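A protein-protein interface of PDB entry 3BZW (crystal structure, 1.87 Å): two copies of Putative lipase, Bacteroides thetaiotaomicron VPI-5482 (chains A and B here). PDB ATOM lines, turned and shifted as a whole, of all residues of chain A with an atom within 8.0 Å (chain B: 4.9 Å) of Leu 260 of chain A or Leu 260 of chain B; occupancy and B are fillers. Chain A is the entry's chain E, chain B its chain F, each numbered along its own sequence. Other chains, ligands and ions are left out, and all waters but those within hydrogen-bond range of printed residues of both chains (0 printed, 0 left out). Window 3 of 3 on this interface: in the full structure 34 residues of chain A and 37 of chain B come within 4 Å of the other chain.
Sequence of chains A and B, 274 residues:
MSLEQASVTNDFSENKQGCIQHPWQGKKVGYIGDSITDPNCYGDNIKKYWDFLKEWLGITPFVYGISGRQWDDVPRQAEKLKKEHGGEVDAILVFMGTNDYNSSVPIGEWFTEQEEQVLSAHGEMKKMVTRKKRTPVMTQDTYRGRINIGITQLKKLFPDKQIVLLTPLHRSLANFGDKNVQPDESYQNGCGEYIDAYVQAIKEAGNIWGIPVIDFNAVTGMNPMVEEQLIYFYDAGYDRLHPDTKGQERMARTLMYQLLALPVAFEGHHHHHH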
ATOM      1  N   ILE A  20      11.542  -1.544 -19.684  1.00  0.00           N
ATOM      2  CA  ILE A  20      10.133  -1.370 -20.144  1.00  0.00           C
ATOM      3  C   ILE A  20       9.194  -2.393 -19.518  1.00  0.00           C
ATOM      4  O   ILE A  20       9.437  -3.597 -19.577  1.00  0.00           O
ATOM      5  CB  ILE A  20      10.028  -1.484 -21.680  1.00  0.00           C
ATOM      6  CG1 ILE A  20      10.786  -2.722 -22.162  1.00  0.00           C
ATOM      7  CG2 ILE A  20      10.559  -0.216 -22.332  1.00  0.00           C
ATOM      8  CD1 ILE A  20      10.829  -2.871 -23.669  1.00  0.00           C
ATOM      9  N   GLN A  21       8.120  -1.900 -18.912  1.00  0.00           N
ATOM     10  CA  GLN A  21       7.138  -2.764 -18.273  1.00  0.00           C
ATOM     11  C   GLN A  21       5.980  -3.017 -19.234  1.00  0.00           C
ATOM     12  O   GLN A  21       5.684  -2.188 -20.088  1.00  0.00           O
ATOM     13  CB  GLN A  21       6.625  -2.108 -16.990  1.00  0.00           C
ATOM     14  CG  GLN A  21       7.729  -1.716 -16.012  1.00  0.00           C
ATOM     15  CD  GLN A  21       8.537  -2.907 -15.523  1.00  0.00           C
ATOM     16  OE1 GLN A  21       8.010  -3.795 -14.850  1.00  0.00           O
ATOM     17  NE2 GLN A  21       9.823  -2.933 -15.862  1.00  0.00           N
ATOM     18  N   HIS A  22       5.330  -4.166 -19.097  1.00  0.00           N
ATOM     19  CA  HIS A  22       4.209  -4.497 -19.963  1.00  0.00           C
ATOM     20  C   HIS A  22       3.090  -3.482 -19.719  1.00  0.00           C
ATOM     21  O   HIS A  22       2.616  -3.331 -18.596  1.00  0.00           O
ATOM     22  CB  HIS A  22       3.720  -5.915 -19.662  1.00  0.00           C
ATOM     23  CG  HIS A  22       2.873  -6.499 -20.746  1.00  0.00           C
ATOM     24  ND1 HIS A  22       1.694  -5.920 -21.163  1.00  0.00           N
ATOM     25  CD2 HIS A  22       3.048  -7.596 -21.519  1.00  0.00           C
ATOM     26  CE1 HIS A  22       1.179  -6.635 -22.146  1.00  0.00           C
ATOM     27  NE2 HIS A  22       1.982  -7.657 -22.383  1.00  0.00           N
ATOM     28  N   PRO A  23       2.658  -2.767 -20.772  1.00  0.00           N
ATOM     29  CA  PRO A  23       1.595  -1.764 -20.641  1.00  0.00           C
ATOM     30  C   PRO A  23       0.265  -2.261 -20.086  1.00  0.00           C
ATOM     31  O   PRO A  23      -0.533  -1.471 -19.583  1.00  0.00           O
ATOM     32  CB  PRO A  23       1.460  -1.214 -22.063  1.00  0.00           C
ATOM     33  CG  PRO A  23       1.877  -2.375 -22.921  1.00  0.00           C
ATOM     34  CD  PRO A  23       3.080  -2.902 -22.176  1.00  0.00           C
ATOM     35  N   TRP A  24       0.024  -3.563 -20.168  1.00  0.00           N
ATOM     36  CA  TRP A  24      -1.229  -4.116 -19.679  1.00  0.00           C
ATOM     37  C   TRP A  24      -1.111  -4.658 -18.263  1.00  0.00           C
ATOM     38  O   TRP A  24      -2.106  -5.037 -17.648  1.00  0.00           O
ATOM     39  CB  TRP A  24      -1.718  -5.206 -20.640  1.00  0.00           C
ATOM     40  CG  TRP A  24      -2.074  -4.651 -21.982  1.00  0.00           C
ATOM     41  CD1 TRP A  24      -1.238  -4.017 -22.859  1.00  0.00           C
ATOM     42  CD2 TRP A  24      -3.379  -4.606 -22.570  1.00  0.00           C
ATOM     43  NE1 TRP A  24      -1.946  -3.572 -23.952  1.00  0.00           N
ATOM     44  CE2 TRP A  24      -3.262  -3.921 -23.801  1.00  0.00           C
ATOM     45  CE3 TRP A  24      -4.640  -5.077 -22.174  1.00  0.00           C
ATOM     46  CZ2 TRP A  24      -4.360  -3.693 -24.638  1.00  0.00           C
ATOM     47  CZ3 TRP A  24      -5.733  -4.848 -23.010  1.00  0.00           C
ATOM     48  CH2 TRP A  24      -5.583  -4.162 -24.226  1.00  0.00           C
ATOM     49  N   LEU A  57      -0.022 -11.441 -15.681  1.00  0.00           N
ATOM     50  CA  LEU A  57       0.125  -9.985 -15.676  1.00  0.00           C
ATOM     51  C   LEU A  57      -0.699  -9.228 -14.647  1.00  0.00           C
ATOM     52  O   LEU A  57      -0.686  -7.997 -14.633  1.00  0.00           O
ATOM     53  CB  LEU A  57      -0.192  -9.435 -17.067  1.00  0.00           C
ATOM     54  CG  LEU A  57       0.755  -9.885 -18.180  1.00  0.00           C
ATOM     55  CD1 LEU A  57       0.256  -9.356 -19.513  1.00  0.00           C
ATOM     56  CD2 LEU A  57       2.170  -9.380 -17.897  1.00  0.00           C
ATOM     57  N   ILE A 214      -5.931  -7.362 -33.639  1.00  0.00           N
ATOM     58  CA  ILE A 214      -4.893  -8.369 -33.502  1.00  0.00           C
ATOM     59  C   ILE A 214      -5.400  -9.562 -34.299  1.00  0.00           C
ATOM     60  O   ILE A 214      -6.438 -10.137 -33.969  1.00  0.00           O
ATOM     61  CB  ILE A 214      -4.682  -8.771 -32.035  1.00  0.00           C
ATOM     62  CG1 ILE A 214      -4.119  -7.581 -31.254  1.00  0.00           C
ATOM     63  CG2 ILE A 214      -3.727  -9.955 -31.956  1.00  0.00           C
ATOM     64  CD1 ILE A 214      -3.916  -7.863 -29.786  1.00  0.00           C
ATOM     65  N   THR A 254       0.103 -15.847 -26.564  1.00  0.00           N
ATOM     66  CA  THR A 254       0.171 -15.105 -27.815  1.00  0.00           C
ATOM     67  C   THR A 254      -0.302 -13.670 -27.559  1.00  0.00           C
ATOM     68  O   THR A 254       0.338 -12.706 -27.982  1.00  0.00           O
ATOM     69  CB  THR A 254      -0.735 -15.740 -28.898  1.00  0.00           C
ATOM     70  OG1 THR A 254      -0.235 -17.035 -29.245  1.00  0.00           O
ATOM     71  CG2 THR A 254      -0.770 -14.867 -30.146  1.00  0.00           C
ATOM     72  N   LEU A 255      -1.428 -13.539 -26.863  1.00  0.00           N
ATOM     73  CA  LEU A 255      -1.984 -12.227 -26.547  1.00  0.00           C
ATOM     74  C   LEU A 255      -1.010 -11.405 -25.721  1.00  0.00           C
ATOM     75  O   LEU A 255      -0.829 -10.212 -25.956  1.00  0.00           O
ATOM     76  CB  LEU A 255      -3.299 -12.367 -25.769  1.00  0.00           C
ATOM     77  CG  LEU A 255      -4.614 -12.032 -26.478  1.00  0.00           C
ATOM     78  CD1 LEU A 255      -5.767 -12.219 -25.496  1.00  0.00           C
ATOM     79  CD2 LEU A 255      -4.592 -10.600 -27.001  1.00  0.00           C
ATOM     80  N   MET A 256      -0.382 -12.047 -24.747  1.00  0.00           N
ATOM     81  CA  MET A 256       0.563 -11.352 -23.892  1.00  0.00           C
ATOM     82  C   MET A 256       1.590 -10.550 -24.682  1.00  0.00           C
ATOM     83  O   MET A 256       1.810  -9.372 -24.406  1.00  0.00           O
ATOM     84  CB  MET A 256       1.285 -12.347 -22.992  1.00  0.00           C
ATOM     85  CG  MET A 256       2.376 -11.726 -22.148  1.00  0.00           C
ATOM     86  SD  MET A 256       2.867 -12.915 -20.718  1.00  0.00           S
ATOM     87  CE  MET A 256       1.291 -12.670 -19.662  1.00  0.00           C
ATOM     88  N   TYR A 257       2.212 -11.181 -25.671  1.00  0.00           N
ATOM     89  CA  TYR A 257       3.223 -10.493 -26.455  1.00  0.00           C
ATOM     90  C   TYR A 257       2.673  -9.617 -27.577  1.00  0.00           C
ATOM     91  O   TYR A 257       3.308  -8.636 -27.966  1.00  0.00           O
ATOM     92  CB  TYR A 257       4.238 -11.514 -26.965  1.00  0.00           C
ATOM     93  CG  TYR A 257       5.030 -12.101 -25.813  1.00  0.00           C
ATOM     94  CD1 TYR A 257       6.088 -11.393 -25.234  1.00  0.00           C
ATOM     95  CD2 TYR A 257       4.660 -13.315 -25.237  1.00  0.00           C
ATOM     96  CE1 TYR A 257       6.751 -11.880 -24.104  1.00  0.00           C
ATOM     97  CE2 TYR A 257       5.312 -13.806 -24.112  1.00  0.00           C
ATOM     98  CZ  TYR A 257       6.352 -13.087 -23.549  1.00  0.00           C
ATOM     99  OH  TYR A 257       6.972 -13.570 -22.418  1.00  0.00           O
ATOM    100  N   GLN A 258       1.484  -9.950 -28.077  1.00  0.00           N
ATOM    101  CA  GLN A 258       0.855  -9.154 -29.128  1.00  0.00           C
ATOM    102  C   GLN A 258       0.363  -7.825 -28.546  1.00  0.00           C
ATOM    103  O   GLN A 258       0.378  -6.795 -29.217  1.00  0.00           O
ATOM    104  CB  GLN A 258      -0.328  -9.915 -29.738  1.00  0.00           C
ATOM    105  CG  GLN A 258       0.062 -11.090 -30.627  1.00  0.00           C
ATOM    106  CD  GLN A 258       0.543 -10.643 -31.995  1.00  0.00           C
ATOM    107  OE1 GLN A 258      -0.190  -9.988 -32.732  1.00  0.00           O
ATOM    108  NE2 GLN A 258       1.773 -10.997 -32.341  1.00  0.00           N
ATOM    109  N   LEU A 259      -0.074  -7.853 -27.292  1.00  0.00           N
ATOM    110  CA  LEU A 259      -0.570  -6.645 -26.631  1.00  0.00           C
ATOM    111  C   LEU A 259       0.549  -5.707 -26.193  1.00  0.00           C
ATOM    112  O   LEU A 259       0.299  -4.583 -25.758  1.00  0.00           O
ATOM    113  CB  LEU A 259      -1.414  -7.021 -25.412  1.00  0.00           C
ATOM    114  CG  LEU A 259      -2.713  -7.771 -25.709  1.00  0.00           C
ATOM    115  CD1 LEU A 259      -3.371  -8.165 -24.401  1.00  0.00           C
ATOM    116  CD2 LEU A 259      -3.641  -6.900 -26.543  1.00  0.00           C
ATOM    117  N   LEU A 260       1.785  -6.180 -26.304  1.00  0.00           N
ATOM    118  CA  LEU A 260       2.950  -5.393 -25.924  1.00  0.00           C
ATOM    119  C   LEU A 260       3.062  -4.145 -26.803  1.00  0.00           C
ATOM    120  O   LEU A 260       3.618  -3.127 -26.388  1.00  0.00           O
ATOM    121  CB  LEU A 260       4.206  -6.258 -26.072  1.00  0.00           C
ATOM    122  CG  LEU A 260       5.553  -5.733 -25.579  1.00  0.00           C
ATOM    123  CD1 LEU A 260       5.437  -5.286 -24.127  1.00  0.00           C
ATOM    124  CD2 LEU A 260       6.597  -6.838 -25.720  1.00  0.00           C
ATOM    125  N   ALA A 261       2.508  -4.223 -28.009  1.00  0.00           N
ATOM    126  CA  ALA A 261       2.564  -3.110 -28.958  1.00  0.00           C
ATOM    127  C   ALA A 261       1.498  -2.033 -28.760  1.00  0.00           C
ATOM    128  O   ALA A 261       1.475  -1.043 -29.495  1.00  0.00           O
ATOM    129  CB  ALA A 261       2.483  -3.652 -30.385  1.00  0.00           C
ATOM    130  N   LEU A 262       0.625  -2.217 -27.771  1.00  0.00           N
ATOM    131  CA  LEU A 262      -0.448  -1.261 -27.507  1.00  0.00           C
ATOM    132  C   LEU A 262      -0.479  -0.768 -26.063  1.00  0.00           C
ATOM    133  O   LEU A 262      -0.408  -1.557 -25.122  1.00  0.00           O
ATOM    134  CB  LEU A 262      -1.802  -1.897 -27.834  1.00  0.00           C
ATOM    135  CG  LEU A 262      -2.011  -2.327 -29.285  1.00  0.00           C
ATOM    136  CD1 LEU A 262      -3.224  -3.245 -29.388  1.00  0.00           C
ATOM    137  CD2 LEU A 262      -2.183  -1.084 -30.155  1.00  0.00           C
ATOM    138  N   PRO A 263      -0.604   0.551 -25.870  1.00  0.00           N
ATOM    139  CA  PRO A 263      -0.647   1.107 -24.518  1.00  0.00           C
ATOM    140  C   PRO A 263      -2.043   0.971 -23.927  1.00  0.00           C
ATOM    141  O   PRO A 263      -3.016   0.743 -24.658  1.00  0.00           O
ATOM    142  CB  PRO A 263      -0.271   2.563 -24.743  1.00  0.00           C
ATOM    143  CG  PRO A 263      -0.956   2.857 -26.040  1.00  0.00           C
ATOM    144  CD  PRO A 263      -0.617   1.627 -26.878  1.00  0.00           C
ATOM    145  N   HIS B  22      13.944  -0.229 -24.501  1.00  0.00           N
ATOM    146  CA  HIS B  22      13.280   0.320 -25.676  1.00  0.00           C
ATOM    147  C   HIS B  22      14.338   0.725 -26.694  1.00  0.00           C
ATOM    148  O   HIS B  22      15.218   1.525 -26.397  1.00  0.00           O
ATOM    149  CB  HIS B  22      12.427   1.530 -25.298  1.00  0.00           C
ATOM    150  CG  HIS B  22      11.382   1.865 -26.315  1.00  0.00           C
ATOM    151  ND1 HIS B  22      11.691   2.198 -27.616  1.00  0.00           N
ATOM    152  CD2 HIS B  22      10.031   1.882 -26.233  1.00  0.00           C
ATOM    153  CE1 HIS B  22      10.575   2.406 -28.292  1.00  0.00           C
ATOM    154  NE2 HIS B  22       9.553   2.221 -27.476  1.00  0.00           N
ATOM    155  N   PRO B  23      14.262   0.171 -27.913  1.00  0.00           N
ATOM    156  CA  PRO B  23      15.232   0.482 -28.969  1.00  0.00           C
ATOM    157  C   PRO B  23      15.327   1.951 -29.384  1.00  0.00           C
ATOM    158  O   PRO B  23      16.333   2.370 -29.961  1.00  0.00           O
ATOM    159  CB  PRO B  23      14.788  -0.422 -30.120  1.00  0.00           C
ATOM    160  CG  PRO B  23      13.305  -0.524 -29.914  1.00  0.00           C
ATOM    161  CD  PRO B  23      13.203  -0.722 -28.418  1.00  0.00           C
ATOM    162  N   MET B 256       4.832   4.992 -28.953  1.00  0.00           N
ATOM    163  CA  MET B 256       5.826   4.432 -28.042  1.00  0.00           C
ATOM    164  C   MET B 256       5.873   2.907 -28.063  1.00  0.00           C
ATOM    165  O   MET B 256       6.948   2.315 -28.148  1.00  0.00           O
ATOM    166  CB  MET B 256       5.573   4.911 -26.608  1.00  0.00           C
ATOM    167  CG  MET B 256       6.605   4.396 -25.607  1.00  0.00           C
ATOM    168  SD  MET B 256       6.526   5.250 -23.867  1.00  0.00           S
ATOM    169  CE  MET B 256       6.311   3.683 -22.772  1.00  0.00           C
ATOM    170  N   TYR B 257       4.715   2.262 -28.001  1.00  0.00           N
ATOM    171  CA  TYR B 257       4.693   0.802 -28.004  1.00  0.00           C
ATOM    172  C   TYR B 257       4.741   0.186 -29.398  1.00  0.00           C
ATOM    173  O   TYR B 257       5.184  -0.948 -29.561  1.00  0.00           O
ATOM    174  CB  TYR B 257       3.484   0.310 -27.206  1.00  0.00           C
ATOM    175  CG  TYR B 257       3.639   0.632 -25.736  1.00  0.00           C
ATOM    176  CD1 TYR B 257       4.394  -0.188 -24.900  1.00  0.00           C
ATOM    177  CD2 TYR B 257       3.110   1.807 -25.199  1.00  0.00           C
ATOM    178  CE1 TYR B 257       4.627   0.149 -23.568  1.00  0.00           C
ATOM    179  CE2 TYR B 257       3.338   2.159 -23.868  1.00  0.00           C
ATOM    180  CZ  TYR B 257       4.099   1.322 -23.060  1.00  0.00           C
ATOM    181  OH  TYR B 257       4.336   1.663 -21.743  1.00  0.00           O
ATOM    182  N   GLN B 258       4.307   0.935 -30.404  1.00  0.00           N
ATOM    183  CA  GLN B 258       4.345   0.435 -31.774  1.00  0.00           C
ATOM    184  C   GLN B 258       5.787   0.423 -32.288  1.00  0.00           C
ATOM    185  O   GLN B 258       6.159  -0.427 -33.096  1.00  0.00           O
ATOM    186  CB  GLN B 258       3.469   1.310 -32.683  1.00  0.00           C
ATOM    187  CG  GLN B 258       1.966   1.165 -32.453  1.00  0.00           C
ATOM    188  CD  GLN B 258       1.392  -0.113 -33.049  1.00  0.00           C
ATOM    189  OE1 GLN B 258       0.853  -0.966 -32.337  1.00  0.00           O
ATOM    190  NE2 GLN B 258       1.499  -0.245 -34.364  1.00  0.00           N
ATOM    191  N   LEU B 259       6.598   1.364 -31.811  1.00  0.00           N
ATOM    192  CA  LEU B 259       8.002   1.455 -32.230  1.00  0.00           C
ATOM    193  C   LEU B 259       8.884   0.409 -31.553  1.00  0.00           C
ATOM    194  O   LEU B 259      10.029   0.198 -31.947  1.00  0.00           O
ATOM    195  CB  LEU B 259       8.556   2.855 -31.936  1.00  0.00           C
ATOM    196  CG  LEU B 259       7.995   3.993 -32.793  1.00  0.00           C
ATOM    197  CD1 LEU B 259       8.597   5.318 -32.346  1.00  0.00           C
ATOM    198  CD2 LEU B 259       8.319   3.731 -34.256  1.00  0.00           C
ATOM    199  N   LEU B 260       8.346  -0.235 -30.527  1.00  0.00           N
ATOM    200  CA  LEU B 260       9.079  -1.260 -29.798  1.00  0.00           C
ATOM    201  C   LEU B 260       9.475  -2.400 -30.743  1.00  0.00           C
ATOM    202  O   LEU B 260      10.465  -3.090 -30.515  1.00  0.00           O
ATOM    203  CB  LEU B 260       8.206  -1.790 -28.658  1.00  0.00           C
ATOM    204  CG  LEU B 260       8.848  -2.614 -27.545  1.00  0.00           C
ATOM    205  CD1 LEU B 260       9.956  -1.804 -26.872  1.00  0.00           C
ATOM    206  CD2 LEU B 260       7.778  -2.995 -26.523  1.00  0.00           C
ATOM    207  N   ALA B 261       8.706  -2.575 -31.812  1.00  0.00           N
ATOM    208  CA  ALA B 261       8.956  -3.639 -32.787  1.00  0.00           C
ATOM    209  C   ALA B 261      10.033  -3.330 -33.831  1.00  0.00           C
ATOM    210  O   ALA B 261      10.365  -4.186 -34.650  1.00  0.00           O
ATOM    211  CB  ALA B 261       7.648  -4.000 -33.494  1.00  0.00           C
ATOM    212  N   LEU B 262      10.584  -2.118 -33.805  1.00  0.00           N
ATOM    213  CA  LEU B 262      11.600  -1.727 -34.783  1.00  0.00           C
ATOM    214  C   LEU B 262      12.885  -1.211 -34.143  1.00  0.00           C
ATOM    215  O   LEU B 262      12.856  -0.352 -33.268  1.00  0.00           O
ATOM    216  CB  LEU B 262      11.037  -0.647 -35.716  1.00  0.00           C
ATOM    217  CG  LEU B 262       9.835  -1.040 -36.586  1.00  0.00           C
ATOM    218  CD1 LEU B 262       9.235   0.200 -37.212  1.00  0.00           C
ATOM    219  CD2 LEU B 262      10.267  -2.034 -37.664  1.00  0.00           C
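O of Ala 261 of chain A lies close to OE1 of Gln 258 of chain B (2.9 Å).
The indole nitrogen (NE1) of Trp 24 of chain A is in hydrogen-bond range of the backbone carbonyl oxygen (O) of Leu 262 of chain A (2.8 Å). O of Met 256 of chain B sits at hydrogen-bond distance from NE2 of His 22 of chain B.
Among the printed residues, pairs that only touch across the chains: Ala 261 of chain A with Tyr 257 of chain B, Leu 260 of chain A with Tyr 257 of chain B, Ile 20 of chain A with Leu 260 of chain B, Pro 263 of chain A with Tyr 257 of chain B, Leu 260 of chain A with Leu 260 of chain B, Pro 23 of chain A with Tyr 257 of chain B, Leu 262 of chain A with Gln 258 of chain B, Leu 262 of chain A with Tyr 257 of chain B and Ile 20 of chain A with His 22 of chain B.
Printed residues of chain B within 4 Å of Pro 23 of chain A: Tyr 257. Leu 260 of chain A touches just these residues of chain B: Tyr 257 and Leu 260. Of the printed residues of chain B, Pro 263 of chain A touches Tyr 257. Of the printed residues of chain A, His 22 of chain B touches Ile 20. Of the printed residues of chain A, Tyr 257 of chain B touches Pro 23, Leu 260, Ala 261, Leu 262 and Pro 263. Leu 260 of chain B touches just these residues of chain A: Ile 20 (3.5 Å) and Leu 260 (3.7 Å). Ala 261 of chain B touches none of the printed residues of chain A. The nearest printed residue of chain B that does not touch Leu 260 of chain A is Gln 258 of chain B (5.8 Å). The nearest printed residue of chain A that does not touch His 22 of chain B is Leu 260 of chain A (8.1 Å).
Printed residues of chain B that touch a printed residue of chain A: His 22, Tyr 257, Gln 258 and Leu 260. Of the 17 printed residues of chain A, 6 touch a printed residue of chain B. Hydrophobic or aromatic side chains of chain A within 4 Å of the printed part of chain B: Ile 20, Pro 23, Leu 260, Ala 261, Leu 262 and Pro 263. Among the printed residues, no Asp or Glu carboxylate lies within 4 Å of a Lys or Arg side-chain nitrogen of the other chain.
Leu 260 of chain B touches its own counterpart, Leu 260 of chain A. Ala 261 of chain A touches Tyr 257 of chain B, but with the chains exchanged Tyr 257 of chain A does not touch Ala 261 of chain B (8.4 Å). Leu 262 of chain A touches Tyr 257 of chain B, but with the chains exchanged Tyr 257 of chain A does not touch Leu 262 of chain B (11.4 Å). Leu 262 of chain A touches Gln 258 of chain B, but with the chains exchanged Gln 258 of chain A does not touch Leu 262 of chain B (12.1 Å). Of the 10 pairs that touch across the chains among the printed residues, 1 has its exchanged pair printed and touching as well.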
